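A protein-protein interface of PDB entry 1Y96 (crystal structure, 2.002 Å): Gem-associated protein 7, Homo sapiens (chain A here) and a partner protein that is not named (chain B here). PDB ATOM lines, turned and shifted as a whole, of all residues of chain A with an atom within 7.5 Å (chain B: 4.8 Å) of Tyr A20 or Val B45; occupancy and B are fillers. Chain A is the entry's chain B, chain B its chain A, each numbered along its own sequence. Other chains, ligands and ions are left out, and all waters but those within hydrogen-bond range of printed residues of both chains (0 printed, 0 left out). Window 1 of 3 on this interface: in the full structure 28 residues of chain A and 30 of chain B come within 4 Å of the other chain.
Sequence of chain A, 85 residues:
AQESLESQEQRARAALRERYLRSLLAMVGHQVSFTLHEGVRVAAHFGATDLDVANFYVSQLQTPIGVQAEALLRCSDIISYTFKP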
ATOM      1  N   ALA A  14       0.005 -23.851  20.252  1.00  0.00           N
ATOM      2  CA  ALA A  14       0.778 -22.800  19.597  1.00  0.00           C
ATOM      3  C   ALA A  14       0.105 -21.431  19.726  1.00  0.00           C
ATOM      4  O   ALA A  14       0.787 -20.455  20.008  1.00  0.00           O
ATOM      5  CB  ALA A  14       1.034 -23.144  18.096  1.00  0.00           C
ATOM      6  N   ALA A  15      -1.208 -21.354  19.511  1.00  0.00           N
ATOM      7  CA  ALA A  15      -1.933 -20.084  19.625  1.00  0.00           C
ATOM      8  C   ALA A  15      -1.910 -19.534  21.048  1.00  0.00           C
ATOM      9  O   ALA A  15      -1.667 -18.349  21.249  1.00  0.00           O
ATOM     10  CB  ALA A  15      -3.397 -20.220  19.099  1.00  0.00           C
ATOM     11  N   LEU A  16      -2.122 -20.392  22.040  1.00  0.00           N
ATOM     12  CA  LEU A  16      -2.072 -19.998  23.444  1.00  0.00           C
ATOM     13  C   LEU A  16      -0.702 -19.492  23.821  1.00  0.00           C
ATOM     14  O   LEU A  16      -0.543 -18.516  24.570  1.00  0.00           O
ATOM     15  CB  LEU A  16      -2.435 -21.199  24.332  1.00  0.00           C
ATOM     16  CG  LEU A  16      -3.896 -21.677  24.306  1.00  0.00           C
ATOM     17  CD1 LEU A  16      -4.049 -23.013  25.004  1.00  0.00           C
ATOM     18  CD2 LEU A  16      -4.819 -20.689  24.976  1.00  0.00           C
ATOM     19  N   ARG A  17       0.325 -20.184  23.311  1.00  0.00           N
ATOM     20  CA  ARG A  17       1.675 -19.858  23.654  1.00  0.00           C
ATOM     21  C   ARG A  17       2.084 -18.535  23.022  1.00  0.00           C
ATOM     22  O   ARG A  17       2.724 -17.704  23.660  1.00  0.00           O
ATOM     23  CB  ARG A  17       2.582 -21.028  23.220  1.00  0.00           C
ATOM     24  CG  ARG A  17       4.020 -20.828  23.504  1.00  0.00           C
ATOM     25  CD  ARG A  17       4.363 -20.762  24.965  1.00  0.00           C
ATOM     26  NE  ARG A  17       5.801 -20.765  25.102  1.00  0.00           N
ATOM     27  CZ  ARG A  17       6.473 -20.537  26.208  1.00  0.00           C
ATOM     28  NH1 ARG A  17       5.850 -20.277  27.366  1.00  0.00           N
ATOM     29  NH2 ARG A  17       7.797 -20.573  26.156  1.00  0.00           N
ATOM     30  N   GLU A  18       1.690 -18.320  21.779  1.00  0.00           N
ATOM     31  CA  GLU A  18       2.061 -17.106  21.066  1.00  0.00           C
ATOM     32  C   GLU A  18       1.466 -15.901  21.799  1.00  0.00           C
ATOM     33  O   GLU A  18       2.128 -14.864  21.971  1.00  0.00           O
ATOM     34  CB  GLU A  18       1.540 -17.195  19.620  1.00  0.00           C
ATOM     35  CG  GLU A  18       1.938 -16.032  18.702  1.00  0.00           C
ATOM     36  CD  GLU A  18       1.033 -14.810  18.862  1.00  0.00           C
ATOM     37  OE1 GLU A  18      -0.184 -14.987  19.128  1.00  0.00           O
ATOM     38  OE2 GLU A  18       1.537 -13.668  18.728  1.00  0.00           O
ATOM     39  N   ARG A  19       0.221 -16.049  22.252  1.00  0.00           N
ATOM     40  CA  ARG A  19      -0.452 -14.979  22.989  1.00  0.00           C
ATOM     41  C   ARG A  19       0.245 -14.717  24.308  1.00  0.00           C
ATOM     42  O   ARG A  19       0.399 -13.560  24.689  1.00  0.00           O
ATOM     43  CB  ARG A  19      -1.946 -15.285  23.212  1.00  0.00           C
ATOM     44  CG  ARG A  19      -2.752 -15.461  21.921  1.00  0.00           C
ATOM     45  CD  ARG A  19      -4.135 -16.104  22.107  1.00  0.00           C
ATOM     46  NE  ARG A  19      -4.959 -15.199  22.883  1.00  0.00           N
ATOM     47  CZ  ARG A  19      -5.708 -14.204  22.391  1.00  0.00           C
ATOM     48  NH1 ARG A  19      -5.805 -13.979  21.087  1.00  0.00           N
ATOM     49  NH2 ARG A  19      -6.379 -13.425  23.227  1.00  0.00           N
ATOM     50  N   TYR A  20       0.708 -15.775  24.973  1.00  0.00           N
ATOM     51  CA  TYR A  20       1.396 -15.634  26.254  1.00  0.00           C
ATOM     52  C   TYR A  20       2.723 -14.885  26.093  1.00  0.00           C
ATOM     53  O   TYR A  20       3.056 -13.988  26.892  1.00  0.00           O
ATOM     54  CB  TYR A  20       1.618 -16.994  26.948  1.00  0.00           C
ATOM     55  CG  TYR A  20       2.164 -16.814  28.352  1.00  0.00           C
ATOM     56  CD1 TYR A  20       1.398 -16.155  29.329  1.00  0.00           C
ATOM     57  CD2 TYR A  20       3.436 -17.236  28.686  1.00  0.00           C
ATOM     58  CE1 TYR A  20       1.868 -15.966  30.583  1.00  0.00           C
ATOM     59  CE2 TYR A  20       3.933 -17.041  29.952  1.00  0.00           C
ATOM     60  CZ  TYR A  20       3.143 -16.393  30.906  1.00  0.00           C
ATOM     61  OH  TYR A  20       3.604 -16.183  32.182  1.00  0.00           O
ATOM     62  N   LEU A  21       3.490 -15.252  25.061  1.00  0.00           N
ATOM     63  CA  LEU A  21       4.764 -14.597  24.815  1.00  0.00           C
ATOM     64  C   LEU A  21       4.535 -13.110  24.481  1.00  0.00           C
ATOM     65  O   LEU A  21       5.269 -12.244  24.939  1.00  0.00           O
ATOM     66  CB  LEU A  21       5.551 -15.292  23.707  1.00  0.00           C
ATOM     67  CG  LEU A  21       6.048 -16.702  24.045  1.00  0.00           C
ATOM     68  CD1 LEU A  21       6.616 -17.351  22.802  1.00  0.00           C
ATOM     69  CD2 LEU A  21       7.075 -16.695  25.141  1.00  0.00           C
ATOM     70  N   ARG A  22       3.503 -12.833  23.706  1.00  0.00           N
ATOM     71  CA  ARG A  22       3.103 -11.458  23.410  1.00  0.00           C
ATOM     72  C   ARG A  22       2.792 -10.667  24.692  1.00  0.00           C
ATOM     73  O   ARG A  22       3.224  -9.524  24.832  1.00  0.00           O
ATOM     74  CB  ARG A  22       1.908 -11.460  22.452  1.00  0.00           C
ATOM     75  CG  ARG A  22       1.476 -10.109  21.949  1.00  0.00           C
ATOM     76  CD  ARG A  22       0.738 -10.171  20.587  1.00  0.00           C
ATOM     77  NE  ARG A  22       1.696 -10.046  19.486  1.00  0.00           N
ATOM     78  CZ  ARG A  22       1.487  -9.384  18.340  1.00  0.00           C
ATOM     79  NH1 ARG A  22       0.323  -8.776  18.092  1.00  0.00           N
ATOM     80  NH2 ARG A  22       2.458  -9.332  17.427  1.00  0.00           N
ATOM     81  N   SER A  23       2.086 -11.276  25.635  1.00  0.00           N
ATOM     82  CA  SER A  23       1.759 -10.625  26.905  1.00  0.00           C
ATOM     83  C   SER A  23       3.015 -10.330  27.722  1.00  0.00           C
ATOM     84  O   SER A  23       3.087  -9.283  28.358  1.00  0.00           O
ATOM     85  CB  SER A  23       0.750 -11.433  27.741  1.00  0.00           C
ATOM     86  OG  SER A  23       1.310 -12.589  28.351  1.00  0.00           O
ATOM     87  N   LEU A  24       4.009 -11.233  27.701  1.00  0.00           N
ATOM     88  CA  LEU A  24       5.261 -11.007  28.424  1.00  0.00           C
ATOM     89  C   LEU A  24       6.068  -9.896  27.733  1.00  0.00           C
ATOM     90  O   LEU A  24       6.642  -9.024  28.382  1.00  0.00           O
ATOM     91  CB  LEU A  24       6.106 -12.305  28.529  1.00  0.00           C
ATOM     92  CG  LEU A  24       5.555 -13.432  29.418  1.00  0.00           C
ATOM     93  CD1 LEU A  24       6.448 -14.694  29.337  1.00  0.00           C
ATOM     94  CD2 LEU A  24       5.397 -12.968  30.832  1.00  0.00           C
ATOM     95  N   LEU A  25       6.108  -9.917  26.410  1.00  0.00           N
ATOM     96  CA  LEU A  25       6.875  -8.914  25.673  1.00  0.00           C
ATOM     97  C   LEU A  25       6.311  -7.509  25.927  1.00  0.00           C
ATOM     98  O   LEU A  25       7.072  -6.563  26.057  1.00  0.00           O
ATOM     99  CB  LEU A  25       6.927  -9.239  24.177  1.00  0.00           C
ATOM    100  CG  LEU A  25       7.889 -10.389  23.787  1.00  0.00           C
ATOM    101  CD1 LEU A  25       7.544 -10.933  22.393  1.00  0.00           C
ATOM    102  CD2 LEU A  25       9.309  -9.915  23.809  1.00  0.00           C
ATOM    103  N   ALA A  26       4.993  -7.389  26.053  1.00  0.00           N
ATOM    104  CA  ALA A  26       4.360  -6.097  26.381  1.00  0.00           C
ATOM    105  C   ALA A  26       4.675  -5.586  27.789  1.00  0.00           C
ATOM    106  O   ALA A  26       4.518  -4.394  28.074  1.00  0.00           O
ATOM    107  CB  ALA A  26       2.858  -6.194  26.216  1.00  0.00           C
ATOM    108  N   THR A  49      11.756 -13.604  30.746  1.00  0.00           N
ATOM    109  CA  THR A  49      11.728 -14.923  31.375  1.00  0.00           C
ATOM    110  C   THR A  49      12.480 -15.884  30.478  1.00  0.00           C
ATOM    111  O   THR A  49      12.727 -15.589  29.307  1.00  0.00           O
ATOM    112  CB  THR A  49      10.292 -15.479  31.606  1.00  0.00           C
ATOM    113  OG1 THR A  49       9.723 -15.938  30.374  1.00  0.00           O
ATOM    114  CG2 THR A  49       9.322 -14.407  32.047  1.00  0.00           C
ATOM    115  N   ASP A  50      12.799 -17.047  31.005  1.00  0.00           N
ATOM    116  CA  ASP A  50      13.195 -18.143  30.119  1.00  0.00           C
ATOM    117  C   ASP A  50      11.958 -18.802  29.499  1.00  0.00           C
ATOM    118  O   ASP A  50      10.809 -18.566  29.937  1.00  0.00           O
ATOM    119  CB  ASP A  50      14.143 -19.128  30.804  1.00  0.00           C
ATOM    120  CG  ASP A  50      13.590 -19.714  32.071  1.00  0.00           C
ATOM    121  OD1 ASP A  50      14.152 -19.433  33.155  1.00  0.00           O
ATOM    122  OD2 ASP A  50      12.657 -20.534  32.075  1.00  0.00           O
ATOM    123  N   LEU A  51      12.183 -19.563  28.432  1.00  0.00           N
ATOM    124  CA  LEU A  51      11.102 -20.211  27.689  1.00  0.00           C
ATOM    125  C   LEU A  51      10.353 -21.261  28.545  1.00  0.00           C
ATOM    126  O   LEU A  51       9.157 -21.437  28.393  1.00  0.00           O
ATOM    127  CB  LEU A  51      11.639 -20.819  26.376  1.00  0.00           C
ATOM    128  CG  LEU A  51      11.268 -20.189  25.012  1.00  0.00           C
ATOM    129  CD1 LEU A  51      11.003 -18.722  25.028  1.00  0.00           C
ATOM    130  CD2 LEU A  51      12.318 -20.520  23.959  1.00  0.00           C
ATOM    131  N   VAL A  53       9.616 -20.696  31.462  1.00  0.00           N
ATOM    132  CA  VAL A  53       8.974 -19.818  32.433  1.00  0.00           C
ATOM    133  C   VAL A  53       9.310 -20.259  33.867  1.00  0.00           C
ATOM    134  O   VAL A  53       8.470 -20.254  34.730  1.00  0.00           O
ATOM    135  CB  VAL A  53       7.432 -19.723  32.236  1.00  0.00           C
ATOM    136  CG1 VAL A  53       6.877 -18.483  32.942  1.00  0.00           C
ATOM    137  CG2 VAL A  53       7.064 -19.658  30.745  1.00  0.00           C
ATOM    138  N   PHE A  56      11.945 -15.304  36.252  1.00  0.00           N
ATOM    139  CA  PHE A  56      11.811 -13.944  35.763  1.00  0.00           C
ATOM    140  C   PHE A  56      13.092 -13.165  36.024  1.00  0.00           C
ATOM    141  O   PHE A  56      13.594 -13.139  37.155  1.00  0.00           O
ATOM    142  CB  PHE A  56      10.648 -13.224  36.466  1.00  0.00           C
ATOM    143  CG  PHE A  56       9.274 -13.598  35.950  1.00  0.00           C
ATOM    144  CD1 PHE A  56       9.025 -14.795  35.321  1.00  0.00           C
ATOM    145  CD2 PHE A  56       8.237 -12.717  36.069  1.00  0.00           C
ATOM    146  CE1 PHE A  56       7.732 -15.109  34.854  1.00  0.00           C
ATOM    147  CE2 PHE A  56       6.961 -13.026  35.595  1.00  0.00           C
ATOM    148  CZ  PHE A  56       6.715 -14.208  35.004  1.00  0.00           C
ATOM    149  N   CYS A  75       9.896 -18.647  39.571  1.00  0.00           N
ATOM    150  CA  CYS A  75       8.450 -18.633  39.382  1.00  0.00           C
ATOM    151  C   CYS A  75       7.756 -19.531  40.419  1.00  0.00           C
ATOM    152  O   CYS A  75       6.621 -19.268  40.787  1.00  0.00           O
ATOM    153  CB  CYS A  75       8.073 -18.987  37.925  1.00  0.00           C
ATOM    154  SG  CYS A  75       8.691 -17.715  36.731  1.00  0.00           S
ATOM    155  N   TYR A  81       1.512 -11.951  39.292  1.00  0.00           N
ATOM    156  CA  TYR A  81       2.194 -10.719  38.903  1.00  0.00           C
ATOM    157  C   TYR A  81       1.218  -9.816  38.196  1.00  0.00           C
ATOM    158  O   TYR A  81       0.386 -10.286  37.438  1.00  0.00           O
ATOM    159  CB  TYR A  81       3.401 -11.002  37.989  1.00  0.00           C
ATOM    160  CG  TYR A  81       3.106 -11.768  36.697  1.00  0.00           C
ATOM    161  CD1 TYR A  81       2.825 -11.101  35.519  1.00  0.00           C
ATOM    162  CD2 TYR A  81       3.173 -13.161  36.655  1.00  0.00           C
ATOM    163  CE1 TYR A  81       2.563 -11.793  34.336  1.00  0.00           C
ATOM    164  CE2 TYR A  81       2.927 -13.863  35.476  1.00  0.00           C
ATOM    165  CZ  TYR A  81       2.637 -13.166  34.309  1.00  0.00           C
ATOM    166  OH  TYR A  81       2.375 -13.847  33.139  1.00  0.00           O
ATOM    167  N   PHE A  83       0.689  -5.732  36.283  1.00  0.00           N
ATOM    168  CA  PHE A  83       1.191  -4.454  35.843  1.00  0.00           C
ATOM    169  C   PHE A  83       0.131  -3.700  35.066  1.00  0.00           C
ATOM    170  O   PHE A  83      -0.928  -4.241  34.767  1.00  0.00           O
ATOM    171  CB  PHE A  83       2.457  -4.654  34.993  1.00  0.00           C
ATOM    172  CG  PHE A  83       2.203  -4.995  33.566  1.00  0.00           C
ATOM    173  CD1 PHE A  83       2.436  -4.073  32.565  1.00  0.00           C
ATOM    174  CD2 PHE A  83       1.757  -6.252  33.203  1.00  0.00           C
ATOM    175  CE1 PHE A  83       2.241  -4.410  31.253  1.00  0.00           C
ATOM    176  CE2 PHE A  83       1.546  -6.573  31.880  1.00  0.00           C
ATOM    177  CZ  PHE A  83       1.800  -5.659  30.912  1.00  0.00           C
ATOM    178  N   TRP B  33     -10.799 -10.843  32.795  1.00  0.00           N
ATOM    179  CA  TRP B  33     -11.080 -11.377  31.470  1.00  0.00           C
ATOM    180  C   TRP B  33      -9.868 -12.162  30.947  1.00  0.00           C
ATOM    181  O   TRP B  33      -8.753 -11.648  30.943  1.00  0.00           O
ATOM    182  CB  TRP B  33     -11.402 -10.242  30.509  1.00  0.00           C
ATOM    183  CG  TRP B  33     -12.646  -9.487  30.919  1.00  0.00           C
ATOM    184  CD1 TRP B  33     -12.719  -8.388  31.743  1.00  0.00           C
ATOM    185  CD2 TRP B  33     -13.995  -9.796  30.546  1.00  0.00           C
ATOM    186  NE1 TRP B  33     -14.033  -7.998  31.892  1.00  0.00           N
ATOM    187  CE2 TRP B  33     -14.837  -8.834  31.166  1.00  0.00           C
ATOM    188  CE3 TRP B  33     -14.582 -10.769  29.727  1.00  0.00           C
ATOM    189  CZ2 TRP B  33     -16.226  -8.828  31.001  1.00  0.00           C
ATOM    190  CZ3 TRP B  33     -15.973 -10.775  29.580  1.00  0.00           C
ATOM    191  CH2 TRP B  33     -16.776  -9.805  30.221  1.00  0.00           C
ATOM    192  N   VAL B  34     -10.084 -13.379  30.480  1.00  0.00           N
ATOM    193  CA  VAL B  34      -8.951 -14.249  30.091  1.00  0.00           C
ATOM    194  C   VAL B  34      -8.410 -13.836  28.733  1.00  0.00           C
ATOM    195  O   VAL B  34      -9.128 -13.827  27.736  1.00  0.00           O
ATOM    196  CB  VAL B  34      -9.355 -15.704  30.117  1.00  0.00           C
ATOM    197  CG1 VAL B  34      -8.130 -16.655  29.781  1.00  0.00           C
ATOM    198  CG2 VAL B  34      -9.907 -16.033  31.482  1.00  0.00           C
ATOM    199  N   LEU B  35      -7.140 -13.453  28.711  1.00  0.00           N
ATOM    200  CA  LEU B  35      -6.404 -13.208  27.479  1.00  0.00           C
ATOM    201  C   LEU B  35      -5.819 -14.511  26.903  1.00  0.00           C
ATOM    202  O   LEU B  35      -5.872 -14.748  25.708  1.00  0.00           O
ATOM    203  CB  LEU B  35      -5.261 -12.217  27.769  1.00  0.00           C
ATOM    204  CG  LEU B  35      -4.777 -11.403  26.585  1.00  0.00           C
ATOM    205  CD1 LEU B  35      -5.934 -10.591  25.959  1.00  0.00           C
ATOM    206  CD2 LEU B  35      -3.631 -10.486  27.011  1.00  0.00           C
ATOM    207  N   THR B  36      -5.214 -15.320  27.762  1.00  0.00           N
ATOM    208  CA  THR B  36      -4.691 -16.637  27.380  1.00  0.00           C
ATOM    209  C   THR B  36      -4.321 -17.455  28.607  1.00  0.00           C
ATOM    210  O   THR B  36      -4.389 -16.979  29.744  1.00  0.00           O
ATOM    211  CB  THR B  36      -3.445 -16.501  26.452  1.00  0.00           C
ATOM    212  OG1 THR B  36      -3.139 -17.769  25.849  1.00  0.00           O
ATOM    213  CG2 THR B  36      -2.172 -16.092  27.233  1.00  0.00           C
ATOM    214  N   ASP B  38      -0.877 -19.950  29.357  1.00  0.00           N
ATOM    215  CA  ASP B  38       0.368 -20.498  28.835  1.00  0.00           C
ATOM    216  C   ASP B  38       0.357 -22.027  28.905  1.00  0.00           C
ATOM    217  O   ASP B  38       0.283 -22.582  29.986  1.00  0.00           O
ATOM    218  CB  ASP B  38       1.541 -19.960  29.629  1.00  0.00           C
ATOM    219  CG  ASP B  38       2.866 -20.524  29.147  1.00  0.00           C
ATOM    220  OD1 ASP B  38       3.767 -20.773  29.973  1.00  0.00           O
ATOM    221  OD2 ASP B  38       3.080 -20.743  27.952  1.00  0.00           O
ATOM    222  N   SER B  41       3.475 -23.474  31.359  1.00  0.00           N
ATOM    223  CA  SER B  41       3.427 -23.290  32.821  1.00  0.00           C
ATOM    224  C   SER B  41       2.003 -23.371  33.374  1.00  0.00           C
ATOM    225  O   SER B  41       1.820 -23.450  34.581  1.00  0.00           O
ATOM    226  CB  SER B  41       3.956 -21.909  33.166  1.00  0.00           C
ATOM    227  OG  SER B  41       3.144 -20.944  32.536  1.00  0.00           O
ATOM    228  N   ASN B  43       0.203 -20.788  33.412  1.00  0.00           N
ATOM    229  CA  ASN B  43      -0.070 -19.430  33.896  1.00  0.00           C
ATOM    230  C   ASN B  43      -1.277 -18.863  33.172  1.00  0.00           C
ATOM    231  O   ASN B  43      -1.356 -18.915  31.921  1.00  0.00           O
ATOM    232  CB  ASN B  43       1.124 -18.490  33.667  1.00  0.00           C
ATOM    233  CG  ASN B  43       2.347 -18.892  34.450  1.00  0.00           C
ATOM    234  OD1 ASN B  43       2.308 -19.826  35.259  1.00  0.00           O
ATOM    235  ND2 ASN B  43       3.451 -18.197  34.217  1.00  0.00           N
ATOM    236  N   ILE B  44      -2.218 -18.298  33.928  1.00  0.00           N
ATOM    237  CA  ILE B  44      -3.393 -17.674  33.330  1.00  0.00           C
ATOM    238  C   ILE B  44      -3.220 -16.173  33.304  1.00  0.00           C
ATOM    239  O   ILE B  44      -2.816 -15.568  34.283  1.00  0.00           O
ATOM    240  CB  ILE B  44      -4.676 -18.000  34.108  1.00  0.00           C
ATOM    241  CG1 ILE B  44      -4.722 -19.457  34.507  1.00  0.00           C
ATOM    242  CG2 ILE B  44      -5.897 -17.661  33.272  1.00  0.00           C
ATOM    243  CD1 ILE B  44      -5.795 -19.758  35.562  1.00  0.00           C
ATOM    244  N   VAL B  45      -3.554 -15.557  32.191  1.00  0.00           N
ATOM    245  CA  VAL B  45      -3.399 -14.128  32.058  1.00  0.00           C
ATOM    246  C   VAL B  45      -4.790 -13.475  32.022  1.00  0.00           C
ATOM    247  O   VAL B  45      -5.590 -13.806  31.151  1.00  0.00           O
ATOM    248  CB  VAL B  45      -2.614 -13.762  30.794  1.00  0.00           C
ATOM    249  CG1 VAL B  45      -2.451 -12.270  30.710  1.00  0.00           C
ATOM    250  CG2 VAL B  45      -1.203 -14.492  30.796  1.00  0.00           C
ATOM    251  N   LEU B  46      -5.045 -12.569  32.973  1.00  0.00           N
ATOM    252  CA  LEU B  46      -6.303 -11.808  33.067  1.00  0.00           C
ATOM    253  C   LEU B  46      -6.131 -10.327  32.796  1.00  0.00           C
ATOM    254  O   LEU B  46      -5.133  -9.733  33.189  1.00  0.00           O
ATOM    255  CB  LEU B  46      -6.907 -11.964  34.463  1.00  0.00           C
ATOM    256  CG  LEU B  46      -7.176 -13.373  34.967  1.00  0.00           C
ATOM    257  CD1 LEU B  46      -7.790 -13.359  36.366  1.00  0.00           C
ATOM    258  CD2 LEU B  46      -8.058 -14.127  34.008  1.00  0.00           C
ATOM    259  N   VAL B  47      -7.108  -9.735  32.115  1.00  0.00           N
ATOM    260  CA  VAL B  47      -7.183  -8.299  31.895  1.00  0.00           C
ATOM    261  C   VAL B  47      -8.297  -7.735  32.798  1.00  0.00           C
ATOM    262  O   VAL B  47      -9.388  -8.307  32.884  1.00  0.00           O
ATOM    263  CB  VAL B  47      -7.519  -7.960  30.428  1.00  0.00           C
ATOM    264  CG1 VAL B  47      -7.731  -6.462  30.246  1.00  0.00           C
ATOM    265  CG2 VAL B  47      -6.424  -8.418  29.502  1.00  0.00           C
ATOM    266  N   VAL B  57      -3.074  -5.913  33.709  1.00  0.00           N
ATOM    267  CA  VAL B  57      -2.880  -7.268  33.216  1.00  0.00           C
ATOM    268  C   VAL B  57      -2.237  -8.063  34.341  1.00  0.00           C
ATOM    269  O   VAL B  57      -1.227  -7.632  34.936  1.00  0.00           O
ATOM    270  CB  VAL B  57      -1.989  -7.263  31.982  1.00  0.00           C
ATOM    271  CG1 VAL B  57      -1.603  -8.714  31.543  1.00  0.00           C
ATOM    272  CG2 VAL B  57      -2.661  -6.508  30.836  1.00  0.00           C
ATOM    273  N   THR B  58      -2.799  -9.228  34.627  1.00  0.00           N
ATOM    274  CA  THR B  58      -2.378 -10.056  35.748  1.00  0.00           C
ATOM    275  C   THR B  58      -2.127 -11.498  35.289  1.00  0.00           C
ATOM    276  O   THR B  58      -2.972 -12.100  34.625  1.00  0.00           O
ATOM    277  CB  THR B  58      -3.469 -10.040  36.837  1.00  0.00           C
ATOM    278  OG1 THR B  58      -3.625  -8.701  37.331  1.00  0.00           O
ATOM    279  CG2 THR B  58      -3.079 -10.864  38.057  1.00  0.00           C
ATOM    280  N   GLY B  59      -0.974 -12.047  35.648  1.00  0.00           N
ATOM    281  CA  GLY B  59      -0.711 -13.462  35.444  1.00  0.00           C
ATOM    282  C   GLY B  59      -0.801 -14.189  36.767  1.00  0.00           C
ATOM    283  O   GLY B  59      -0.259 -13.723  37.752  1.00  0.00           O
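Arg A19 touches Thr B36. Tyr A20 touches Thr B36 (N to CG2, 3.7 Å). Asp B38 touches Tyr A20. Tyr A20 touches Val B45 (CE1 to CG2, 3.4 Å). Val B45 touches Ser A23 (CG2 to OG, 3.99 Å). CG2 of Val A53 touches OD1 of Asp B38, 3.6 Å away. ND2 of Asn B43 touches CG1 of Val A53, at 3.7 Å. O of Tyr A81 touches O of Val B57, at 3.99 Å. Thr B58 touches Tyr A81 (CA to O, 3.2 Å).
The backbone NH (N) of Gly B59 is in hydrogen-bond range of the backbone carbonyl oxygen (O) of Tyr A81 (2.9 Å). The backbone carbonyl oxygen (O) of Leu B35 sits at hydrogen-bond distance from the guanidinium group (NH2) of Arg A19, 2.9 Å away. The guanidinium group (NH1) of Arg A17 is in salt-bridge range of the side-chain carboxylate (OD2) of Asp B38, 2.9 Å away. The side-chain amide nitrogen (ND2) of Asn B43 lies within hydrogen-bond range of the side-chain hydroxyl (OH) of Tyr A20, 2.9 Å away. The backbone NH of Val B57 lies within hydrogen-bond range of the backbone carbonyl oxygen of Phe A83, at 2.9 Å. The side-chain hydroxyl (OG1) of Thr B36 sits at hydrogen-bond distance from the backbone carbonyl oxygen (O) of Leu A16 (3.0 Å).
Leu A25 touches none of the printed residues of chain B. Of the printed residues of chain B, Val A53 touches Asp B38 (3.6 Å) and Asn B43 (3.7 Å). Printed residues of chain B within 4 Å of Phe A83: Val B57. Of the printed residues of chain A, Val B45 touches Tyr A20 and Ser A23. Printed residues of chain A within 4 Å of Thr B58: Tyr A81 (3.2 Å). The nearest residue of chain B that does not touch Tyr A20 is Ser B41 (4.7 Å). The nearest printed residue of chain A that does not touch Leu B35 is Ser A23 (4.5 Å).
Of the 14 printed residues of chain B, 8 touch a printed residue of chain A. Hydrophobic or aromatic side chains of chain B within 4 Å of the printed part of chain A: Leu B35, Val B45 and Val B57. Of the 21 printed residues of chain A, 8 touch a printed residue of chain B. Hydrophobic or aromatic side chains of chain A within 4 Å of the printed part of chain B: Leu A16, Tyr A20, Val A53, Tyr A81 and Phe A83. Among the printed residues, 15 pairs touch across the chains.
The side-chain hydroxyl (OG) of Ser B41 lies close to the side-chain amide oxygen (OD1) of Asn B43 (3.1 Å). OD1 of Asp B38 lies within hydrogen-bond range of OG of Ser B41, at 2.6 Å. OD2 of Asp A50 sits at hydrogen-bond distance from N of Val A53. O of Tyr A20 sits at hydrogen-bond distance from OG of Ser A23. The backbone NH (N) of Val B45 is in hydrogen-bond range of the backbone carbonyl oxygen (O) of Thr B36 (3.0 Å). N of Asp B38 lies within hydrogen-bond range of O of Asn B43, 2.8 Å away.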
